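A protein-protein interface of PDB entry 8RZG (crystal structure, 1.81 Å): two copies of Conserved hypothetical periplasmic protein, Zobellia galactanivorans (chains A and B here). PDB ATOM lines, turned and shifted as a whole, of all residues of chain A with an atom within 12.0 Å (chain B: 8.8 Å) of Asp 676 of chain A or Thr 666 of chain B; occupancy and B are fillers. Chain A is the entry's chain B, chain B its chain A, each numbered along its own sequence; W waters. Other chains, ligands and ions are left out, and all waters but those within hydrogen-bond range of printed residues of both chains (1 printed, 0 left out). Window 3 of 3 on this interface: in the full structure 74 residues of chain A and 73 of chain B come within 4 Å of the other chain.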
ATOM      1  N   SER A 672       4.760  16.435   4.434  1.00  0.00           N
ATOM      2  CA  SER A 672       6.178  16.189   4.672  1.00  0.00           C
ATOM      3  C   SER A 672       6.423  15.777   6.118  1.00  0.00           C
ATOM      4  O   SER A 672       5.654  16.123   7.017  1.00  0.00           O
ATOM      5  CB  SER A 672       7.035  17.443   4.394  1.00  0.00           C
ATOM      6  OG  SER A 672       6.759  18.008   3.128  1.00  0.00           O
ATOM      7  N   LEU A 673       7.526  15.069   6.341  1.00  0.00           N
ATOM      8  CA  LEU A 673       7.966  14.693   7.682  1.00  0.00           C
ATOM      9  C   LEU A 673       9.275  15.411   7.971  1.00  0.00           C
ATOM     10  O   LEU A 673      10.306  15.096   7.371  1.00  0.00           O
ATOM     11  CB  LEU A 673       8.139  13.181   7.809  1.00  0.00           C
ATOM     12  CG  LEU A 673       8.809  12.655   9.083  1.00  0.00           C
ATOM     13  CD1 LEU A 673       8.032  13.063  10.331  1.00  0.00           C
ATOM     14  CD2 LEU A 673       8.955  11.143   9.005  1.00  0.00           C
ATOM     15  N   HIS A 674       9.238  16.371   8.889  1.00  0.00           N
ATOM     16  CA  HIS A 674      10.465  16.996   9.363  1.00  0.00           C
ATOM     17  C   HIS A 674      11.034  16.179  10.514  1.00  0.00           C
ATOM     18  O   HIS A 674      10.331  15.896  11.489  1.00  0.00           O
ATOM     19  CB  HIS A 674      10.235  18.428   9.840  1.00  0.00           C
ATOM     20  CG  HIS A 674      11.388  18.966  10.629  1.00  0.00           C
ATOM     21  ND1 HIS A 674      12.565  19.371  10.037  1.00  0.00           N
ATOM     22  CD2 HIS A 674      11.573  19.103  11.964  1.00  0.00           C
ATOM     23  CE1 HIS A 674      13.417  19.757  10.972  1.00  0.00           C
ATOM     24  NE2 HIS A 674      12.837  19.609  12.151  1.00  0.00           N
ATOM     25  N   MET A 675      12.300  15.810  10.404  1.00  0.00           N
ATOM     26  CA  MET A 675      13.005  15.107  11.463  1.00  0.00           C
ATOM     27  C   MET A 675      14.198  15.949  11.890  1.00  0.00           C
ATOM     28  O   MET A 675      15.054  16.278  11.065  1.00  0.00           O
ATOM     29  CB  MET A 675      13.440  13.721  10.996  1.00  0.00           C
ATOM     30  CG  MET A 675      12.328  12.993  10.253  1.00  0.00           C
ATOM     31  SD  MET A 675      12.761  11.317   9.775  1.00  0.00           S
ATOM     32  CE  MET A 675      12.451  10.446  11.307  1.00  0.00           C
ATOM     33  N   ASP A 676      14.241  16.310  13.171  1.00  0.00           N
ATOM     34  CA  ASP A 676      15.368  17.055  13.717  1.00  0.00           C
ATOM     35  C   ASP A 676      16.632  16.229  13.622  1.00  0.00           C
ATOM     36  O   ASP A 676      17.724  16.786  13.496  1.00  0.00           O
ATOM     37  CB  ASP A 676      15.124  17.447  15.177  1.00  0.00           C
ATOM     38  CG  ASP A 676      14.057  18.502  15.327  1.00  0.00           C
ATOM     39  OD1 ASP A 676      13.998  19.419  14.476  1.00  0.00           O
ATOM     40  OD2 ASP A 676      13.277  18.422  16.299  1.00  0.00           O
ATOM     41  OXT ASP A 676      16.576  14.994  13.677  1.00  0.00           O
ATOM     42  N   LEU B 597       9.906   6.956  10.076  1.00  0.00           N
ATOM     43  CA  LEU B 597       9.399   7.299  11.404  1.00  0.00           C
ATOM     44  C   LEU B 597       8.850   6.094  12.161  1.00  0.00           C
ATOM     45  O   LEU B 597       9.299   5.803  13.275  1.00  0.00           O
ATOM     46  CB  LEU B 597       8.313   8.377  11.288  1.00  0.00           C
ATOM     47  CG  LEU B 597       7.700   8.873  12.605  1.00  0.00           C
ATOM     48  CD1 LEU B 597       8.757   9.504  13.500  1.00  0.00           C
ATOM     49  CD2 LEU B 597       6.563   9.847  12.352  1.00  0.00           C
ATOM     50  N   ILE B 634       6.193   9.998  22.972  1.00  0.00           N
ATOM     51  CA  ILE B 634       5.313  11.139  23.195  1.00  0.00           C
ATOM     52  C   ILE B 634       4.889  11.660  21.825  1.00  0.00           C
ATOM     53  O   ILE B 634       5.736  11.869  20.951  1.00  0.00           O
ATOM     54  CB  ILE B 634       6.006  12.246  24.016  1.00  0.00           C
ATOM     55  CG1 ILE B 634       6.522  11.686  25.355  1.00  0.00           C
ATOM     56  CG2 ILE B 634       5.051  13.417  24.222  1.00  0.00           C
ATOM     57  CD1 ILE B 634       7.268  12.709  26.224  1.00  0.00           C
ATOM     58  N   ILE B 648       8.762  21.106  28.307  1.00  0.00           N
ATOM     59  CA  ILE B 648       9.014  20.554  26.984  1.00  0.00           C
ATOM     60  C   ILE B 648       7.813  20.854  26.100  1.00  0.00           C
ATOM     61  O   ILE B 648       6.664  20.692  26.522  1.00  0.00           O
ATOM     62  CB  ILE B 648       9.275  19.041  27.067  1.00  0.00           C
ATOM     63  CG1 ILE B 648      10.422  18.731  28.030  1.00  0.00           C
ATOM     64  CG2 ILE B 648       9.546  18.460  25.673  1.00  0.00           C
ATOM     65  CD1 ILE B 648      11.761  19.192  27.546  1.00  0.00           C
ATOM     66  N   SER B 649       8.068  21.310  24.876  1.00  0.00           N
ATOM     67  CA  SER B 649       7.002  21.560  23.914  1.00  0.00           C
ATOM     68  C   SER B 649       6.953  20.441  22.881  1.00  0.00           C
ATOM     69  O   SER B 649       7.988  20.067  22.313  1.00  0.00           O
ATOM     70  CB  SER B 649       7.199  22.905  23.215  1.00  0.00           C
ATOM     71  OG  SER B 649       6.124  23.144  22.325  1.00  0.00           O
ATOM     72  N   ILE B 650       5.757  19.924  22.624  1.00  0.00           N
ATOM     73  CA  ILE B 650       5.536  18.925  21.584  1.00  0.00           C
ATOM     74  C   ILE B 650       4.827  19.616  20.421  1.00  0.00           C
ATOM     75  O   ILE B 650       3.712  20.126  20.595  1.00  0.00           O
ATOM     76  CB  ILE B 650       4.713  17.726  22.087  1.00  0.00           C
ATOM     77  CG1 ILE B 650       5.249  17.185  23.417  1.00  0.00           C
ATOM     78  CG2 ILE B 650       4.713  16.627  21.025  1.00  0.00           C
ATOM     79  CD1 ILE B 650       6.694  16.674  23.367  1.00  0.00           C
ATOM     80  N   PRO B 651       5.429  19.670  19.234  1.00  0.00           N
ATOM     81  CA  PRO B 651       4.800  20.381  18.117  1.00  0.00           C
ATOM     82  C   PRO B 651       3.477  19.743  17.739  1.00  0.00           C
ATOM     83  O   PRO B 651       3.234  18.562  18.001  1.00  0.00           O
ATOM     84  CB  PRO B 651       5.821  20.234  16.978  1.00  0.00           C
ATOM     85  CG  PRO B 651       7.102  19.846  17.641  1.00  0.00           C
ATOM     86  CD  PRO B 651       6.707  19.056  18.852  1.00  0.00           C
ATOM     87  N   TYR B 653       1.034  17.768  15.556  1.00  0.00           N
ATOM     88  CA  TYR B 653       1.349  16.565  14.774  1.00  0.00           C
ATOM     89  C   TYR B 653       2.832  16.210  14.886  1.00  0.00           C
ATOM     90  O   TYR B 653       3.505  15.897  13.900  1.00  0.00           O
ATOM     91  CB  TYR B 653       0.906  16.731  13.311  1.00  0.00           C
ATOM     92  CG  TYR B 653      -0.554  17.108  13.232  1.00  0.00           C
ATOM     93  CD1 TYR B 653      -1.539  16.255  13.738  1.00  0.00           C
ATOM     94  CD2 TYR B 653      -0.956  18.317  12.680  1.00  0.00           C
ATOM     95  CE1 TYR B 653      -2.876  16.601  13.689  1.00  0.00           C
ATOM     96  CE2 TYR B 653      -2.285  18.672  12.623  1.00  0.00           C
ATOM     97  CZ  TYR B 653      -3.245  17.812  13.130  1.00  0.00           C
ATOM     98  OH  TYR B 653      -4.574  18.171  13.072  1.00  0.00           O
ATOM     99  N   GLY B 654       3.349  16.269  16.114  1.00  0.00           N
ATOM    100  CA  GLY B 654       4.757  16.090  16.379  1.00  0.00           C
ATOM    101  C   GLY B 654       5.003  14.989  17.396  1.00  0.00           C
ATOM    102  O   GLY B 654       4.069  14.399  17.957  1.00  0.00           O
ATOM    103  N   TYR B 655       6.285  14.726  17.630  1.00  0.00           N
ATOM    104  CA  TYR B 655       6.660  13.567  18.426  1.00  0.00           C
ATOM    105  C   TYR B 655       7.984  13.820  19.131  1.00  0.00           C
ATOM    106  O   TYR B 655       8.820  14.628  18.697  1.00  0.00           O
ATOM    107  CB  TYR B 655       6.754  12.296  17.567  1.00  0.00           C
ATOM    108  CG  TYR B 655       7.778  12.421  16.442  1.00  0.00           C
ATOM    109  CD1 TYR B 655       7.435  13.008  15.228  1.00  0.00           C
ATOM    110  CD2 TYR B 655       9.081  11.957  16.602  1.00  0.00           C
ATOM    111  CE1 TYR B 655       8.372  13.138  14.194  1.00  0.00           C
ATOM    112  CE2 TYR B 655      10.020  12.082  15.578  1.00  0.00           C
ATOM    113  CZ  TYR B 655       9.659  12.676  14.380  1.00  0.00           C
ATOM    114  OH  TYR B 655      10.592  12.805  13.363  1.00  0.00           O
ATOM    115  N   ARG B 656       8.163  13.102  20.232  1.00  0.00           N
ATOM    116  CA  ARG B 656       9.392  13.139  21.013  1.00  0.00           C
ATOM    117  C   ARG B 656       9.590  11.723  21.531  1.00  0.00           C
ATOM    118  O   ARG B 656       8.827  11.270  22.392  1.00  0.00           O
ATOM    119  CB  ARG B 656       9.290  14.141  22.156  1.00  0.00           C
ATOM    120  CG  ARG B 656      10.558  14.289  22.932  1.00  0.00           C
ATOM    121  CD  ARG B 656      10.363  15.252  24.083  1.00  0.00           C
ATOM    122  NE  ARG B 656      11.609  15.492  24.798  1.00  0.00           N
ATOM    123  CZ  ARG B 656      12.446  16.491  24.531  1.00  0.00           C
ATOM    124  NH1 ARG B 656      12.179  17.351  23.558  1.00  0.00           N
ATOM    125  NH2 ARG B 656      13.556  16.631  25.243  1.00  0.00           N
ATOM    126  N   ILE B 657      10.571  11.006  20.983  1.00  0.00           N
ATOM    127  CA  ILE B 657      10.668   9.563  21.185  1.00  0.00           C
ATOM    128  C   ILE B 657      12.051   9.219  21.710  1.00  0.00           C
ATOM    129  O   ILE B 657      13.057   9.460  21.031  1.00  0.00           O
ATOM    130  CB  ILE B 657      10.379   8.776  19.898  1.00  0.00           C
ATOM    131  CG1 ILE B 657       9.004   9.152  19.341  1.00  0.00           C
ATOM    132  CG2 ILE B 657      10.483   7.279  20.169  1.00  0.00           C
ATOM    133  CD1 ILE B 657       8.635   8.422  18.056  1.00  0.00           C
ATOM    134  N   GLN B 658      12.100   8.641  22.904  1.00  0.00           N
ATOM    135  CA  GLN B 658      13.350   8.202  23.510  1.00  0.00           C
ATOM    136  C   GLN B 658      13.547   6.727  23.177  1.00  0.00           C
ATOM    137  O   GLN B 658      12.769   5.876  23.621  1.00  0.00           O
ATOM    138  CB  GLN B 658      13.306   8.442  25.015  1.00  0.00           C
ATOM    139  CG  GLN B 658      14.611   8.273  25.758  1.00  0.00           C
ATOM    140  CD  GLN B 658      14.489   8.786  27.180  1.00  0.00           C
ATOM    141  OE1 GLN B 658      13.388   9.118  27.633  1.00  0.00           O
ATOM    142  NE2 GLN B 658      15.613   8.865  27.890  1.00  0.00           N
ATOM    143  N   MET B 659      14.574   6.429  22.392  1.00  0.00           N
ATOM    144  CA  MET B 659      14.860   5.069  21.963  1.00  0.00           C
ATOM    145  C   MET B 659      15.763   4.366  22.971  1.00  0.00           C
ATOM    146  O   MET B 659      16.434   5.001  23.788  1.00  0.00           O
ATOM    147  CB  MET B 659      15.523   5.069  20.583  1.00  0.00           C
ATOM    148  CG  MET B 659      14.703   5.773  19.510  1.00  0.00           C
ATOM    149  SD  MET B 659      13.191   4.892  19.082  1.00  0.00           S
ATOM    150  CE  MET B 659      13.838   3.426  18.270  1.00  0.00           C
ATOM    151  N   SER B 663      19.121   7.541  21.724  1.00  0.00           N
ATOM    152  CA  SER B 663      18.795   8.605  20.790  1.00  0.00           C
ATOM    153  C   SER B 663      17.411   9.169  21.083  1.00  0.00           C
ATOM    154  O   SER B 663      16.523   8.482  21.592  1.00  0.00           O
ATOM    155  CB  SER B 663      18.870   8.111  19.343  1.00  0.00           C
ATOM    156  OG  SER B 663      17.907   7.110  19.069  1.00  0.00           O
ATOM    157  N   LEU B 664      17.239  10.447  20.765  1.00  0.00           N
ATOM    158  CA  LEU B 664      15.975  11.149  20.939  1.00  0.00           C
ATOM    159  C   LEU B 664      15.489  11.576  19.560  1.00  0.00           C
ATOM    160  O   LEU B 664      16.123  12.412  18.908  1.00  0.00           O
ATOM    161  CB  LEU B 664      16.151  12.353  21.867  1.00  0.00           C
ATOM    162  CG  LEU B 664      14.880  13.123  22.232  1.00  0.00           C
ATOM    163  CD1 LEU B 664      14.000  12.318  23.179  1.00  0.00           C
ATOM    164  CD2 LEU B 664      15.225  14.480  22.841  1.00  0.00           C
ATOM    165  N   LYS B 665      14.383  10.994  19.106  1.00  0.00           N
ATOM    166  CA  LYS B 665      13.784  11.369  17.830  1.00  0.00           C
ATOM    167  C   LYS B 665      12.762  12.473  18.069  1.00  0.00           C
ATOM    168  O   LYS B 665      11.799  12.283  18.826  1.00  0.00           O
ATOM    169  CB  LYS B 665      13.109  10.172  17.161  1.00  0.00           C
ATOM    170  CG  LYS B 665      13.901   8.878  17.210  1.00  0.00           C
ATOM    171  CD  LYS B 665      15.222   8.972  16.455  1.00  0.00           C
ATOM    172  CE  LYS B 665      15.948   7.625  16.477  1.00  0.00           C
ATOM    173  NZ  LYS B 665      17.427   7.756  16.308  1.00  0.00           N
ATOM    174  N   THR B 666      12.965  13.620  17.428  1.00  0.00           N
ATOM    175  CA  THR B 666      12.000  14.706  17.487  1.00  0.00           C
ATOM    176  C   THR B 666      11.717  15.201  16.078  1.00  0.00           C
ATOM    177  O   THR B 666      12.584  15.151  15.202  1.00  0.00           O
ATOM    178  CB  THR B 666      12.482  15.884  18.352  1.00  0.00           C
ATOM    179  OG1 THR B 666      13.723  16.376  17.834  1.00  0.00           O
ATOM    180  CG2 THR B 666      12.680  15.456  19.804  1.00  0.00           C
ATOM    181  N   GLY B 667      10.499  15.687  15.878  1.00  0.00           N
ATOM    182  CA  GLY B 667      10.092  16.181  14.580  1.00  0.00           C
ATOM    183  C   GLY B 667       8.588  16.347  14.543  1.00  0.00           C
ATOM    184  O   GLY B 667       7.906  16.234  15.568  1.00  0.00           O
ATOM    185  N   HIS B 668       8.080  16.598  13.337  1.00  0.00           N
ATOM    186  CA  HIS B 668       6.650  16.812  13.164  1.00  0.00           C
ATOM    187  C   HIS B 668       6.315  16.735  11.685  1.00  0.00           C
ATOM    188  O   HIS B 668       7.177  16.925  10.819  1.00  0.00           O
ATOM    189  CB  HIS B 668       6.204  18.168  13.727  1.00  0.00           C
ATOM    190  CG  HIS B 668       6.753  19.338  12.966  1.00  0.00           C
ATOM    191  ND1 HIS B 668       7.974  19.907  13.255  1.00  0.00           N
ATOM    192  CD2 HIS B 668       6.254  20.033  11.917  1.00  0.00           C
ATOM    193  CE1 HIS B 668       8.200  20.909  12.423  1.00  0.00           C
ATOM    194  NE2 HIS B 668       7.173  21.006  11.599  1.00  0.00           N
ATOM    195  N   PHE B 669       5.046  16.459  11.415  1.00  0.00           N
ATOM    196  CA  PHE B 669       4.526  16.510  10.059  1.00  0.00           C
ATOM    197  C   PHE B 669       4.144  17.936   9.681  1.00  0.00           C
ATOM    198  O   PHE B 669       3.688  18.721  10.515  1.00  0.00           O
ATOM    199  CB  PHE B 669       3.300  15.614   9.921  1.00  0.00           C
ATOM    200  CG  PHE B 669       3.594  14.148  10.046  1.00  0.00           C
ATOM    201  CD1 PHE B 669       3.965  13.409   8.934  1.00  0.00           C
ATOM    202  CD2 PHE B 669       3.460  13.500  11.262  1.00  0.00           C
ATOM    203  CE1 PHE B 669       4.221  12.044   9.038  1.00  0.00           C
ATOM    204  CE2 PHE B 669       3.708  12.136  11.372  1.00  0.00           C
ATOM    205  CZ  PHE B 669       4.084  11.412  10.258  1.00  0.00           C
HETATM  206  O   HOH W   1      15.312  13.437  15.536  1.00  0.00           O
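Asp 676 of chain A touches just these residues of chain B: Thr 666 (2.6 Å) and Gly 667 (3.9 Å).
Of the printed residues of chain A, Thr 666 of chain B touches Met 675 (3.8 Å) and Asp 676 (2.6 Å).
No residue of chain A comes within 4 Å of Arg 656 of chain B.
Gly 667 of chain B touches just these residues of chain A: His 674 and Asp 676.
Of the printed residues of chain A, Leu 597 of chain B touches Leu 673.
Printed residues of chain A within 4 Å of Phe 669 of chain B: Ser 672 (3.3 Å).
Gly 654 of chain B touches none of the printed residues of chain A.
Pro 651 of chain B touches none of the printed residues of chain A.
The nearest residue of chain A that does not touch Thr 666 of chain B is His 674 of chain A (4.4 Å).
The nearest printed residue of chain A that does not touch Leu 597 of chain B is Met 675 of chain A (4.4 Å).
O of Tyr 653 of chain B sits at hydrogen-bond distance from N of Phe 669 of chain B (3.0 Å).
The side-chain carboxylate of Asp 676 of chain A lies within hydrogen-bond range of a ring nitrogen (NE2) of His 674 of chain A (2.6 Å).
O of Gly 667 of chain B lies within hydrogen-bond range of N of Tyr 655 of chain B, 3.0 Å away.
No position is printed for both chains.
Of the 11 pairs that touch across the chains among the printed residues, none has its exchanged pair printed and touching as well.
Among the printed residues, merely in contact across the chains: His 674 of chain A with Gly 667 of chain B, Ser 672 of chain A with Phe 669 of chain B, Met 675 of chain A with Tyr 655 of chain B, His 674 of chain A with Tyr 655 of chain B, Leu 673 of chain A with Leu 597 of chain B, Met 675 of chain A with Thr 666 of chain B, Leu 673 of chain A with His 668 of chain B, Leu 673 of chain A with Tyr 655 of chain B and Asp 676 of chain A with Gly 667 of chain B.
Water W1 bridges the chain-end carboxylate (OXT) of Asp 676 of chain A (2.7 Å) and the backbone NH (N) of Thr 666 of chain B (3.0 Å).
OD2 of Asp 676 of chain A lies within hydrogen-bond range of OG1 of Thr 666 of chain B (2.6 Å).
O of His 668 of chain B sits at hydrogen-bond distance from N of His 674 of chain A, at 2.9 Å.
Of the 20 printed residues of chain B, 6 touch a printed residue of chain A.
Printed residues of chain B that touch a printed residue of chain A: Leu 597, Tyr 655, Thr 666, Gly 667, His 668 and Phe 669.
Of the 5 printed residues of chain A, 5 touch a printed residue of chain B.
Hydrophobic or aromatic side chains of chain A within 4 Å of the printed part of chain B: Leu 673, His 674 and Met 675.
Among the printed residues, no Asp or Glu carboxylate lies within 4 Å of a Lys or Arg side-chain nitrogen of the other chain.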
